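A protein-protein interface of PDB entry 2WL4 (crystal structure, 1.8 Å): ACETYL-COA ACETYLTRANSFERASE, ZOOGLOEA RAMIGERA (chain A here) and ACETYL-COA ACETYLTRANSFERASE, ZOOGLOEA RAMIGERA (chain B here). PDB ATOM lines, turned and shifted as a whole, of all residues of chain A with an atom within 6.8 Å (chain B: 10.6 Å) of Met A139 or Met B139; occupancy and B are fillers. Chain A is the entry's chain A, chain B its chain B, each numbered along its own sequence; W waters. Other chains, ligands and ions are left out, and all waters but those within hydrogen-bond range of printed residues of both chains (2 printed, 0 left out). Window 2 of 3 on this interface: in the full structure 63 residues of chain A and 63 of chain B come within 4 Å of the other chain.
N of His A124 sits at hydrogen-bond distance from O of Ala B126, at 2.9 Å.
N of Ala A126 sits at hydrogen-bond distance from O of His B124.
NH2 of Arg B129 lies within salt-bridge range of OD1 of Asp A141.
Water W1 lies within hydrogen-bond range of a ring nitrogen (ND1) of His B124 (2.8 Å), the backbone carbonyl oxygen of Ala B122 (2.8 Å) and the backbone NH of Leu A128 (3.1 Å).
Water W2 bridges a ring nitrogen (ND1) of His A124 and the backbone NH of Leu B128.
Met A139 touches just one residue of chain B: Met B139 (3.4 Å).
Of chain A, only Met A139 comes within 4 Å of Met B139.
Of chain B, only Pro B123, His B124 and Cys B125 come within 4 Å of Cys A125.
Ala A126 touches just these residues of chain B: Pro B123 (3.2 Å) and His B124 (3.0 Å).
No residue of chain B comes within 4 Å of Ile A140.
Printed residues of chain B within 4 Å of Asp A141: Arg B129 (2.7 Å).
Of the printed residues of chain A, His B124 touches Cys A125 (3.2 Å) and Ala A126 (3.0 Å).
Printed residues of chain A within 4 Å of Ala B126: His A124.
Of the printed residues of chain A, Arg B129 touches Asp A141.
Printed residues of chain A within 4 Å of Cys B125: His A124 (3.2 Å) and Cys A125 (3.8 Å).
The nearest residue of chain A that does not touch Met B139 is Leu A128 (4.2 Å).
The nearest printed residue of chain A that does not touch Cys B125 is Ala A126 (5.2 Å).
The backbone NH (N) of Cys A125 sits at hydrogen-bond distance from the backbone carbonyl oxygen (O) of Ile A140, at 2.8 Å.
OG1 of Thr B142 sits at hydrogen-bond distance from O of Pro B123.
N of Ile B140 lies within hydrogen-bond range of O of Cys B125 (2.7 Å).
Printed residues of chain B that touch a printed residue of chain A: Pro B123, His B124, Cys B125, Ala B126, Arg B129 and Met B139.
Hydrophobic or aromatic side chains of chain B within 4 Å of the printed part of chain A: Pro B123 and Met B139.
Of the 9 printed residues of chain A, 5 touch a printed residue of chain B.
Among the printed residues, 9 pairs touch across the chains.
Among the printed residues, Asp or Glu carboxylates within 4 Å of a Lys or Arg side-chain nitrogen of the other chain: Asp A141 with Arg B129 (2.7 Å).
His A124 touches Cys B125 (O to CA, 3.2 Å).
Cys A125 touches Pro B123.
Cys A125 touches His B124 (CA to O, 3.2 Å).
Cys A125 touches Cys B125.
Pro B123 touches Ala A126 (CB to O, 3.2 Å).
CE of Met B139 touches CE of Met A139 (3.4 Å).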
ATOM      1  N   HIS A 124     -16.337  27.172  13.098  1.00  0.00           N
ATOM      2  CA  HIS A 124     -14.964  27.076  12.641  1.00  0.00           C
ATOM      3  C   HIS A 124     -14.162  26.592  13.827  1.00  0.00           C
ATOM      4  O   HIS A 124     -14.540  26.841  14.965  1.00  0.00           O
ATOM      5  CB  HIS A 124     -14.452  28.448  12.196  1.00  0.00           C
ATOM      6  CG  HIS A 124     -14.891  28.838  10.818  1.00  0.00           C
ATOM      7  ND1 HIS A 124     -16.188  29.174  10.523  1.00  0.00           N
ATOM      8  CD2 HIS A 124     -14.188  28.959   9.668  1.00  0.00           C
ATOM      9  CE1 HIS A 124     -16.274  29.483   9.235  1.00  0.00           C
ATOM     10  NE2 HIS A 124     -15.079  29.358   8.698  1.00  0.00           N
ATOM     11  N   CYS A 125     -13.060  25.898  13.582  1.00  0.00           N
ATOM     12  CA  CYS A 125     -12.359  25.285  14.691  1.00  0.00           C
ATOM     13  C   CYS A 125     -10.849  25.239  14.501  1.00  0.00           C
ATOM     14  O   CYS A 125     -10.329  25.496  13.406  1.00  0.00           O
ATOM     15  CB  CYS A 125     -12.915  23.878  14.970  1.00  0.00           C
ATOM     16  SG  CYS A 125     -12.419  22.592  13.794  1.00  0.00           S
ATOM     17  N   ALA A 126     -10.141  24.929  15.579  1.00  0.00           N
ATOM     18  CA  ALA A 126      -8.707  24.706  15.485  1.00  0.00           C
ATOM     19  C   ALA A 126      -8.211  23.968  16.713  1.00  0.00           C
ATOM     20  O   ALA A 126      -8.668  24.227  17.812  1.00  0.00           O
ATOM     21  CB  ALA A 126      -7.972  26.025  15.360  1.00  0.00           C
ATOM     22  N   LEU A 128      -5.812  23.759  19.453  1.00  0.00           N
ATOM     23  CA  LEU A 128      -4.955  24.775  20.072  1.00  0.00           C
ATOM     24  C   LEU A 128      -4.312  24.339  21.395  1.00  0.00           C
ATOM     25  O   LEU A 128      -3.748  25.176  22.111  1.00  0.00           O
ATOM     26  CB  LEU A 128      -5.762  26.053  20.294  1.00  0.00           C
ATOM     27  CG  LEU A 128      -6.236  26.776  19.021  1.00  0.00           C
ATOM     28  CD1 LEU A 128      -7.225  27.874  19.340  1.00  0.00           C
ATOM     29  CD2 LEU A 128      -5.040  27.343  18.274  1.00  0.00           C
ATOM     30  N   PHE A 137      -2.488  30.900  12.088  1.00  0.00           N
ATOM     31  CA  PHE A 137      -2.919  29.504  11.990  1.00  0.00           C
ATOM     32  C   PHE A 137      -4.291  29.439  11.299  1.00  0.00           C
ATOM     33  O   PHE A 137      -4.983  30.451  11.199  1.00  0.00           O
ATOM     34  CB  PHE A 137      -2.927  28.807  13.364  1.00  0.00           C
ATOM     35  CG  PHE A 137      -3.783  29.493  14.393  1.00  0.00           C
ATOM     36  CD1 PHE A 137      -5.136  29.190  14.509  1.00  0.00           C
ATOM     37  CD2 PHE A 137      -3.238  30.440  15.243  1.00  0.00           C
ATOM     38  CE1 PHE A 137      -5.925  29.821  15.458  1.00  0.00           C
ATOM     39  CE2 PHE A 137      -4.023  31.083  16.188  1.00  0.00           C
ATOM     40  CZ  PHE A 137      -5.366  30.773  16.299  1.00  0.00           C
ATOM     41  N   LYS A 138      -4.663  28.263  10.814  1.00  0.00           N
ATOM     42  CA  LYS A 138      -5.945  28.078  10.124  1.00  0.00           C
ATOM     43  C   LYS A 138      -7.118  27.797  11.060  1.00  0.00           C
ATOM     44  O   LYS A 138      -7.076  26.857  11.856  1.00  0.00           O
ATOM     45  CB  LYS A 138      -5.852  26.913   9.139  1.00  0.00           C
ATOM     46  CG  LYS A 138      -5.432  27.285   7.738  1.00  0.00           C
ATOM     47  CD  LYS A 138      -5.275  26.040   6.874  1.00  0.00           C
ATOM     48  CE  LYS A 138      -5.086  26.409   5.411  1.00  0.00           C
ATOM     49  NZ  LYS A 138      -4.496  25.294   4.623  1.00  0.00           N
ATOM     50  N   MET A 139      -8.168  28.606  10.948  1.00  0.00           N
ATOM     51  CA  MET A 139      -9.458  28.238  11.508  1.00  0.00           C
ATOM     52  C   MET A 139     -10.235  27.503  10.419  1.00  0.00           C
ATOM     53  O   MET A 139     -10.441  28.034   9.321  1.00  0.00           O
ATOM     54  CB  MET A 139     -10.226  29.464  11.992  1.00  0.00           C
ATOM     55  CG  MET A 139      -9.654  30.086  13.260  1.00  0.00           C
ATOM     56  SD  MET A 139     -10.037  29.106  14.733  1.00  0.00           S
ATOM     57  CE  MET A 139     -11.703  29.671  15.048  1.00  0.00           C
ATOM     58  N   ILE A 140     -10.646  26.284  10.752  1.00  0.00           N
ATOM     59  CA  ILE A 140     -11.185  25.306   9.808  1.00  0.00           C
ATOM     60  C   ILE A 140     -12.716  25.319   9.862  1.00  0.00           C
ATOM     61  O   ILE A 140     -13.292  25.186  10.927  1.00  0.00           O
ATOM     62  CB  ILE A 140     -10.632  23.894  10.180  1.00  0.00           C
ATOM     63  CG1 ILE A 140      -9.095  23.889  10.052  1.00  0.00           C
ATOM     64  CG2 ILE A 140     -11.281  22.780   9.361  1.00  0.00           C
ATOM     65  CD1 ILE A 140      -8.617  23.984   8.609  1.00  0.00           C
ATOM     66  N   ASP A 141     -13.359  25.511   8.710  1.00  0.00           N
ATOM     67  CA  ASP A 141     -14.805  25.456   8.610  1.00  0.00           C
ATOM     68  C   ASP A 141     -15.251  23.986   8.800  1.00  0.00           C
ATOM     69  O   ASP A 141     -15.013  23.142   7.934  1.00  0.00           O
ATOM     70  CB  ASP A 141     -15.255  26.010   7.242  1.00  0.00           C
ATOM     71  CG  ASP A 141     -16.754  26.186   7.143  1.00  0.00           C
ATOM     72  OD1 ASP A 141     -17.479  25.439   7.848  1.00  0.00           O
ATOM     73  OD2 ASP A 141     -17.226  27.036   6.331  1.00  0.00           O
ATOM     74  N   GLY B  61     -13.166  18.447  13.146  1.00  0.00           N
ATOM     75  CA  GLY B  61     -11.917  18.775  12.476  1.00  0.00           C
ATOM     76  C   GLY B  61     -11.131  17.601  11.924  1.00  0.00           C
ATOM     77  O   GLY B  61     -10.183  17.801  11.172  1.00  0.00           O
ATOM     78  N   ALA B 122      -9.069  17.193  20.261  1.00  0.00           N
ATOM     79  CA  ALA B 122     -10.340  17.930  20.147  1.00  0.00           C
ATOM     80  C   ALA B 122     -10.107  19.440  20.044  1.00  0.00           C
ATOM     81  O   ALA B 122      -9.349  20.004  20.837  1.00  0.00           O
ATOM     82  CB  ALA B 122     -11.239  17.604  21.334  1.00  0.00           C
ATOM     83  N   PRO B 123     -10.736  20.106  19.063  1.00  0.00           N
ATOM     84  CA  PRO B 123     -10.409  21.525  18.898  1.00  0.00           C
ATOM     85  C   PRO B 123     -11.285  22.472  19.714  1.00  0.00           C
ATOM     86  O   PRO B 123     -12.270  22.071  20.332  1.00  0.00           O
ATOM     87  CB  PRO B 123     -10.667  21.744  17.392  1.00  0.00           C
ATOM     88  CG  PRO B 123     -11.878  20.921  17.175  1.00  0.00           C
ATOM     89  CD  PRO B 123     -11.488  19.609  17.891  1.00  0.00           C
ATOM     90  N   HIS B 124     -10.886  23.739  19.737  1.00  0.00           N
ATOM     91  CA  HIS B 124     -11.747  24.803  20.214  1.00  0.00           C
ATOM     92  C   HIS B 124     -12.513  25.312  18.992  1.00  0.00           C
ATOM     93  O   HIS B 124     -12.016  25.233  17.869  1.00  0.00           O
ATOM     94  CB  HIS B 124     -10.901  25.935  20.802  1.00  0.00           C
ATOM     95  CG  HIS B 124     -10.323  25.620  22.149  1.00  0.00           C
ATOM     96  ND1 HIS B 124      -9.356  24.657  22.341  1.00  0.00           N
ATOM     97  CD2 HIS B 124     -10.597  26.132  23.375  1.00  0.00           C
ATOM     98  CE1 HIS B 124      -9.036  24.608  23.624  1.00  0.00           C
ATOM     99  NE2 HIS B 124      -9.779  25.482  24.274  1.00  0.00           N
ATOM    100  N   CYS B 125     -13.696  25.869  19.203  1.00  0.00           N
ATOM    101  CA  CYS B 125     -14.509  26.280  18.066  1.00  0.00           C
ATOM    102  C   CYS B 125     -15.360  27.498  18.347  1.00  0.00           C
ATOM    103  O   CYS B 125     -15.500  27.930  19.495  1.00  0.00           O
ATOM    104  CB  CYS B 125     -15.419  25.128  17.613  1.00  0.00           C
ATOM    105  SG  CYS B 125     -16.805  24.799  18.755  1.00  0.00           S
ATOM    106  N   ALA B 126     -15.922  28.058  17.281  1.00  0.00           N
ATOM    107  CA  ALA B 126     -16.814  29.201  17.401  1.00  0.00           C
ATOM    108  C   ALA B 126     -17.651  29.324  16.146  1.00  0.00           C
ATOM    109  O   ALA B 126     -17.142  29.151  15.053  1.00  0.00           O
ATOM    110  CB  ALA B 126     -16.015  30.490  17.637  1.00  0.00           C
ATOM    111  N   HIS B 127     -18.932  29.623  16.320  1.00  0.00           N
ATOM    112  CA  HIS B 127     -19.813  29.896  15.187  1.00  0.00           C
ATOM    113  C   HIS B 127     -19.640  31.340  14.759  1.00  0.00           C
ATOM    114  O   HIS B 127     -20.020  32.248  15.488  1.00  0.00           O
ATOM    115  CB  HIS B 127     -21.275  29.642  15.557  1.00  0.00           C
ATOM    116  CG  HIS B 127     -22.241  30.006  14.474  1.00  0.00           C
ATOM    117  ND1 HIS B 127     -23.284  30.903  14.663  1.00  0.00           N
ATOM    118  CD2 HIS B 127     -22.304  29.649  13.170  1.00  0.00           C
ATOM    119  CE1 HIS B 127     -23.960  31.033  13.546  1.00  0.00           C
ATOM    120  NE2 HIS B 127     -23.382  30.285  12.611  1.00  0.00           N
ATOM    121  N   LEU B 128     -19.092  31.532  13.562  1.00  0.00           N
ATOM    122  CA  LEU B 128     -18.653  32.841  13.099  1.00  0.00           C
ATOM    123  C   LEU B 128     -19.286  33.268  11.774  1.00  0.00           C
ATOM    124  O   LEU B 128     -18.834  34.242  11.164  1.00  0.00           O
ATOM    125  CB  LEU B 128     -17.134  32.832  12.947  1.00  0.00           C
ATOM    126  CG  LEU B 128     -16.341  32.518  14.225  1.00  0.00           C
ATOM    127  CD1 LEU B 128     -14.866  32.436  13.930  1.00  0.00           C
ATOM    128  CD2 LEU B 128     -16.612  33.592  15.269  1.00  0.00           C
ATOM    129  N   ARG B 129     -20.319  32.544  11.332  1.00  0.00           N
ATOM    130  CA  ARG B 129     -20.958  32.803  10.038  1.00  0.00           C
ATOM    131  C   ARG B 129     -21.795  34.072   9.988  1.00  0.00           C
ATOM    132  O   ARG B 129     -21.775  34.790   8.985  1.00  0.00           O
ATOM    133  CB  ARG B 129     -21.822  31.613   9.595  1.00  0.00           C
ATOM    134  CG  ARG B 129     -21.008  30.501   8.986  1.00  0.00           C
ATOM    135  CD  ARG B 129     -21.870  29.430   8.311  1.00  0.00           C
ATOM    136  NE  ARG B 129     -21.370  28.140   8.745  1.00  0.00           N
ATOM    137  CZ  ARG B 129     -20.308  27.536   8.226  1.00  0.00           C
ATOM    138  NH1 ARG B 129     -19.631  28.108   7.233  1.00  0.00           N
ATOM    139  NH2 ARG B 129     -19.905  26.375   8.725  1.00  0.00           N
ATOM    140  N   VAL B 132     -19.869  38.481  14.380  1.00  0.00           N
ATOM    141  CA  VAL B 132     -20.161  39.027  15.701  1.00  0.00           C
ATOM    142  C   VAL B 132     -20.106  40.553  15.655  1.00  0.00           C
ATOM    143  O   VAL B 132     -19.031  41.151  15.648  1.00  0.00           O
ATOM    144  CB  VAL B 132     -19.208  38.464  16.776  1.00  0.00           C
ATOM    145  CG1 VAL B 132     -19.306  39.271  18.058  1.00  0.00           C
ATOM    146  CG2 VAL B 132     -19.530  36.995  17.039  1.00  0.00           C
ATOM    147  N   GLY B 135     -18.860  43.085  20.790  1.00  0.00           N
ATOM    148  CA  GLY B 135     -18.795  42.428  22.088  1.00  0.00           C
ATOM    149  C   GLY B 135     -17.988  41.139  22.051  1.00  0.00           C
ATOM    150  O   GLY B 135     -17.794  40.551  20.991  1.00  0.00           O
ATOM    151  N   ASP B 136     -17.518  40.692  23.209  1.00  0.00           N
ATOM    152  CA  ASP B 136     -16.688  39.488  23.264  1.00  0.00           C
ATOM    153  C   ASP B 136     -17.477  38.226  22.936  1.00  0.00           C
ATOM    154  O   ASP B 136     -18.711  38.209  23.002  1.00  0.00           O
ATOM    155  CB  ASP B 136     -16.024  39.348  24.641  1.00  0.00           C
ATOM    156  CG  ASP B 136     -15.130  40.528  24.979  1.00  0.00           C
ATOM    157  OD1 ASP B 136     -14.792  41.297  24.060  1.00  0.00           O
ATOM    158  OD2 ASP B 136     -14.766  40.688  26.164  1.00  0.00           O
ATOM    159  N   PHE B 137     -16.749  37.173  22.573  1.00  0.00           N
ATOM    160  CA  PHE B 137     -17.332  35.855  22.357  1.00  0.00           C
ATOM    161  C   PHE B 137     -16.278  34.793  22.651  1.00  0.00           C
ATOM    162  O   PHE B 137     -15.085  35.033  22.494  1.00  0.00           O
ATOM    163  CB  PHE B 137     -17.842  35.709  20.922  1.00  0.00           C
ATOM    164  CG  PHE B 137     -16.757  35.423  19.915  1.00  0.00           C
ATOM    165  CD1 PHE B 137     -16.212  36.440  19.163  1.00  0.00           C
ATOM    166  CD2 PHE B 137     -16.297  34.128  19.712  1.00  0.00           C
ATOM    167  CE1 PHE B 137     -15.221  36.183  18.230  1.00  0.00           C
ATOM    168  CE2 PHE B 137     -15.300  33.866  18.783  1.00  0.00           C
ATOM    169  CZ  PHE B 137     -14.765  34.889  18.044  1.00  0.00           C
ATOM    170  N   LYS B 138     -16.721  33.612  23.056  1.00  0.00           N
ATOM    171  CA  LYS B 138     -15.793  32.557  23.454  1.00  0.00           C
ATOM    172  C   LYS B 138     -15.307  31.709  22.272  1.00  0.00           C
ATOM    173  O   LYS B 138     -16.047  31.469  21.329  1.00  0.00           O
ATOM    174  CB  LYS B 138     -16.477  31.641  24.470  1.00  0.00           C
ATOM    175  CG  LYS B 138     -17.804  32.182  24.991  1.00  0.00           C
ATOM    176  CD  LYS B 138     -18.404  31.295  26.067  1.00  0.00           C
ATOM    177  CE  LYS B 138     -17.857  31.627  27.449  1.00  0.00           C
ATOM    178  NZ  LYS B 138     -18.420  32.896  27.999  1.00  0.00           N
ATOM    179  N   MET B 139     -14.054  31.271  22.322  1.00  0.00           N
ATOM    180  CA  MET B 139     -13.676  30.065  21.605  1.00  0.00           C
ATOM    181  C   MET B 139     -13.957  28.905  22.558  1.00  0.00           C
ATOM    182  O   MET B 139     -13.424  28.859  23.671  1.00  0.00           O
ATOM    183  CB  MET B 139     -12.208  30.098  21.194  1.00  0.00           C
ATOM    184  CG  MET B 139     -11.939  30.996  20.026  1.00  0.00           C
ATOM    185  SD  MET B 139     -12.424  30.244  18.462  1.00  0.00           S
ATOM    186  CE  MET B 139     -11.138  29.006  18.296  1.00  0.00           C
ATOM    187  N   ILE B 140     -14.818  27.998  22.125  1.00  0.00           N
ATOM    188  CA  ILE B 140     -15.327  26.936  22.979  1.00  0.00           C
ATOM    189  C   ILE B 140     -14.491  25.657  22.889  1.00  0.00           C
ATOM    190  O   ILE B 140     -14.235  25.167  21.814  1.00  0.00           O
ATOM    191  CB  ILE B 140     -16.794  26.625  22.612  1.00  0.00           C
ATOM    192  CG1 ILE B 140     -17.644  27.894  22.792  1.00  0.00           C
ATOM    193  CG2 ILE B 140     -17.344  25.513  23.477  1.00  0.00           C
ATOM    194  CD1 ILE B 140     -17.766  28.331  24.232  1.00  0.00           C
ATOM    195  N   ASP B 141     -14.096  25.104  24.031  1.00  0.00           N
ATOM    196  CA  ASP B 141     -13.408  23.822  24.026  1.00  0.00           C
ATOM    197  C   ASP B 141     -14.431  22.712  23.725  1.00  0.00           C
ATOM    198  O   ASP B 141     -15.251  22.391  24.568  1.00  0.00           O
ATOM    199  CB  ASP B 141     -12.721  23.608  25.390  1.00  0.00           C
ATOM    200  CG  ASP B 141     -11.759  22.452  25.387  1.00  0.00           C
ATOM    201  OD1 ASP B 141     -11.980  21.494  24.616  1.00  0.00           O
ATOM    202  OD2 ASP B 141     -10.790  22.485  26.175  1.00  0.00           O
ATOM    203  N   THR B 142     -14.387  22.124  22.530  1.00  0.00           N
ATOM    204  CA  THR B 142     -15.350  21.066  22.181  1.00  0.00           C
ATOM    205  C   THR B 142     -15.305  19.855  23.140  1.00  0.00           C
ATOM    206  O   THR B 142     -16.306  19.171  23.336  1.00  0.00           O
ATOM    207  CB  THR B 142     -15.182  20.571  20.717  1.00  0.00           C
ATOM    208  OG1 THR B 142     -13.837  20.113  20.514  1.00  0.00           O
ATOM    209  CG2 THR B 142     -15.515  21.674  19.724  1.00  0.00           C
ATOM    210  N   MET B 143     -14.142  19.566  23.714  1.00  0.00           N
ATOM    211  CA  MET B 143     -14.049  18.440  24.620  1.00  0.00           C
ATOM    212  C   MET B 143     -14.929  18.690  25.844  1.00  0.00           C
ATOM    213  O   MET B 143     -15.716  17.844  26.241  1.00  0.00           O
ATOM    214  CB  MET B 143     -12.613  18.201  25.034  1.00  0.00           C
ATOM    215  CG  MET B 143     -12.461  17.158  26.128  1.00  0.00           C
ATOM    216  SD  MET B 143     -10.786  17.120  26.818  1.00  0.00           S
ATOM    217  CE  MET B 143     -10.679  18.670  27.698  1.00  0.00           C
ATOM    218  N   ILE B 144     -14.806  19.864  26.431  1.00  0.00           N
ATOM    219  CA  ILE B 144     -15.619  20.216  27.607  1.00  0.00           C
ATOM    220  C   ILE B 144     -17.080  20.348  27.214  1.00  0.00           C
ATOM    221  O   ILE B 144     -17.968  19.762  27.857  1.00  0.00           O
ATOM    222  CB  ILE B 144     -15.155  21.543  28.234  1.00  0.00           C
ATOM    223  CG1 ILE B 144     -13.695  21.442  28.706  1.00  0.00           C
ATOM    224  CG2 ILE B 144     -16.076  21.968  29.378  1.00  0.00           C
ATOM    225  CD1 ILE B 144     -13.439  20.467  29.813  1.00  0.00           C
ATOM    226  N   LYS B 145     -17.334  21.105  26.146  1.00  0.00           N
ATOM    227  CA  LYS B 145     -18.717  21.456  25.780  1.00  0.00           C
ATOM    228  C   LYS B 145     -19.496  20.270  25.247  1.00  0.00           C
ATOM    229  O   LYS B 145     -20.608  20.024  25.676  1.00  0.00           O
ATOM    230  CB  LYS B 145     -18.755  22.577  24.742  1.00  0.00           C
ATOM    231  CG  LYS B 145     -20.153  22.856  24.143  1.00  0.00           C
ATOM    232  CD  LYS B 145     -21.065  23.547  25.178  1.00  0.00           C
ATOM    233  CE  LYS B 145     -22.203  24.348  24.521  1.00  0.00           C
ATOM    234  NZ  LYS B 145     -22.878  25.202  25.540  1.00  0.00           N
ATOM    235  N   ASP B 146     -18.908  19.526  24.314  1.00  0.00           N
ATOM    236  CA  ASP B 146     -19.661  18.429  23.678  1.00  0.00           C
ATOM    237  C   ASP B 146     -19.467  17.078  24.371  1.00  0.00           C
ATOM    238  O   ASP B 146     -20.265  16.166  24.171  1.00  0.00           O
ATOM    239  CB  ASP B 146     -19.318  18.298  22.177  1.00  0.00           C
ATOM    240  CG  ASP B 146     -19.556  19.600  21.403  1.00  0.00           C
ATOM    241  OD1 ASP B 146     -20.472  20.372  21.774  1.00  0.00           O
ATOM    242  OD2 ASP B 146     -18.805  19.861  20.438  1.00  0.00           O
HETATM  243  O   HOH W   1      -8.121  22.533  21.031  1.00  0.00           O
HETATM  244  O   HOH W   2     -18.848  29.270  11.641  1.00  0.00           O
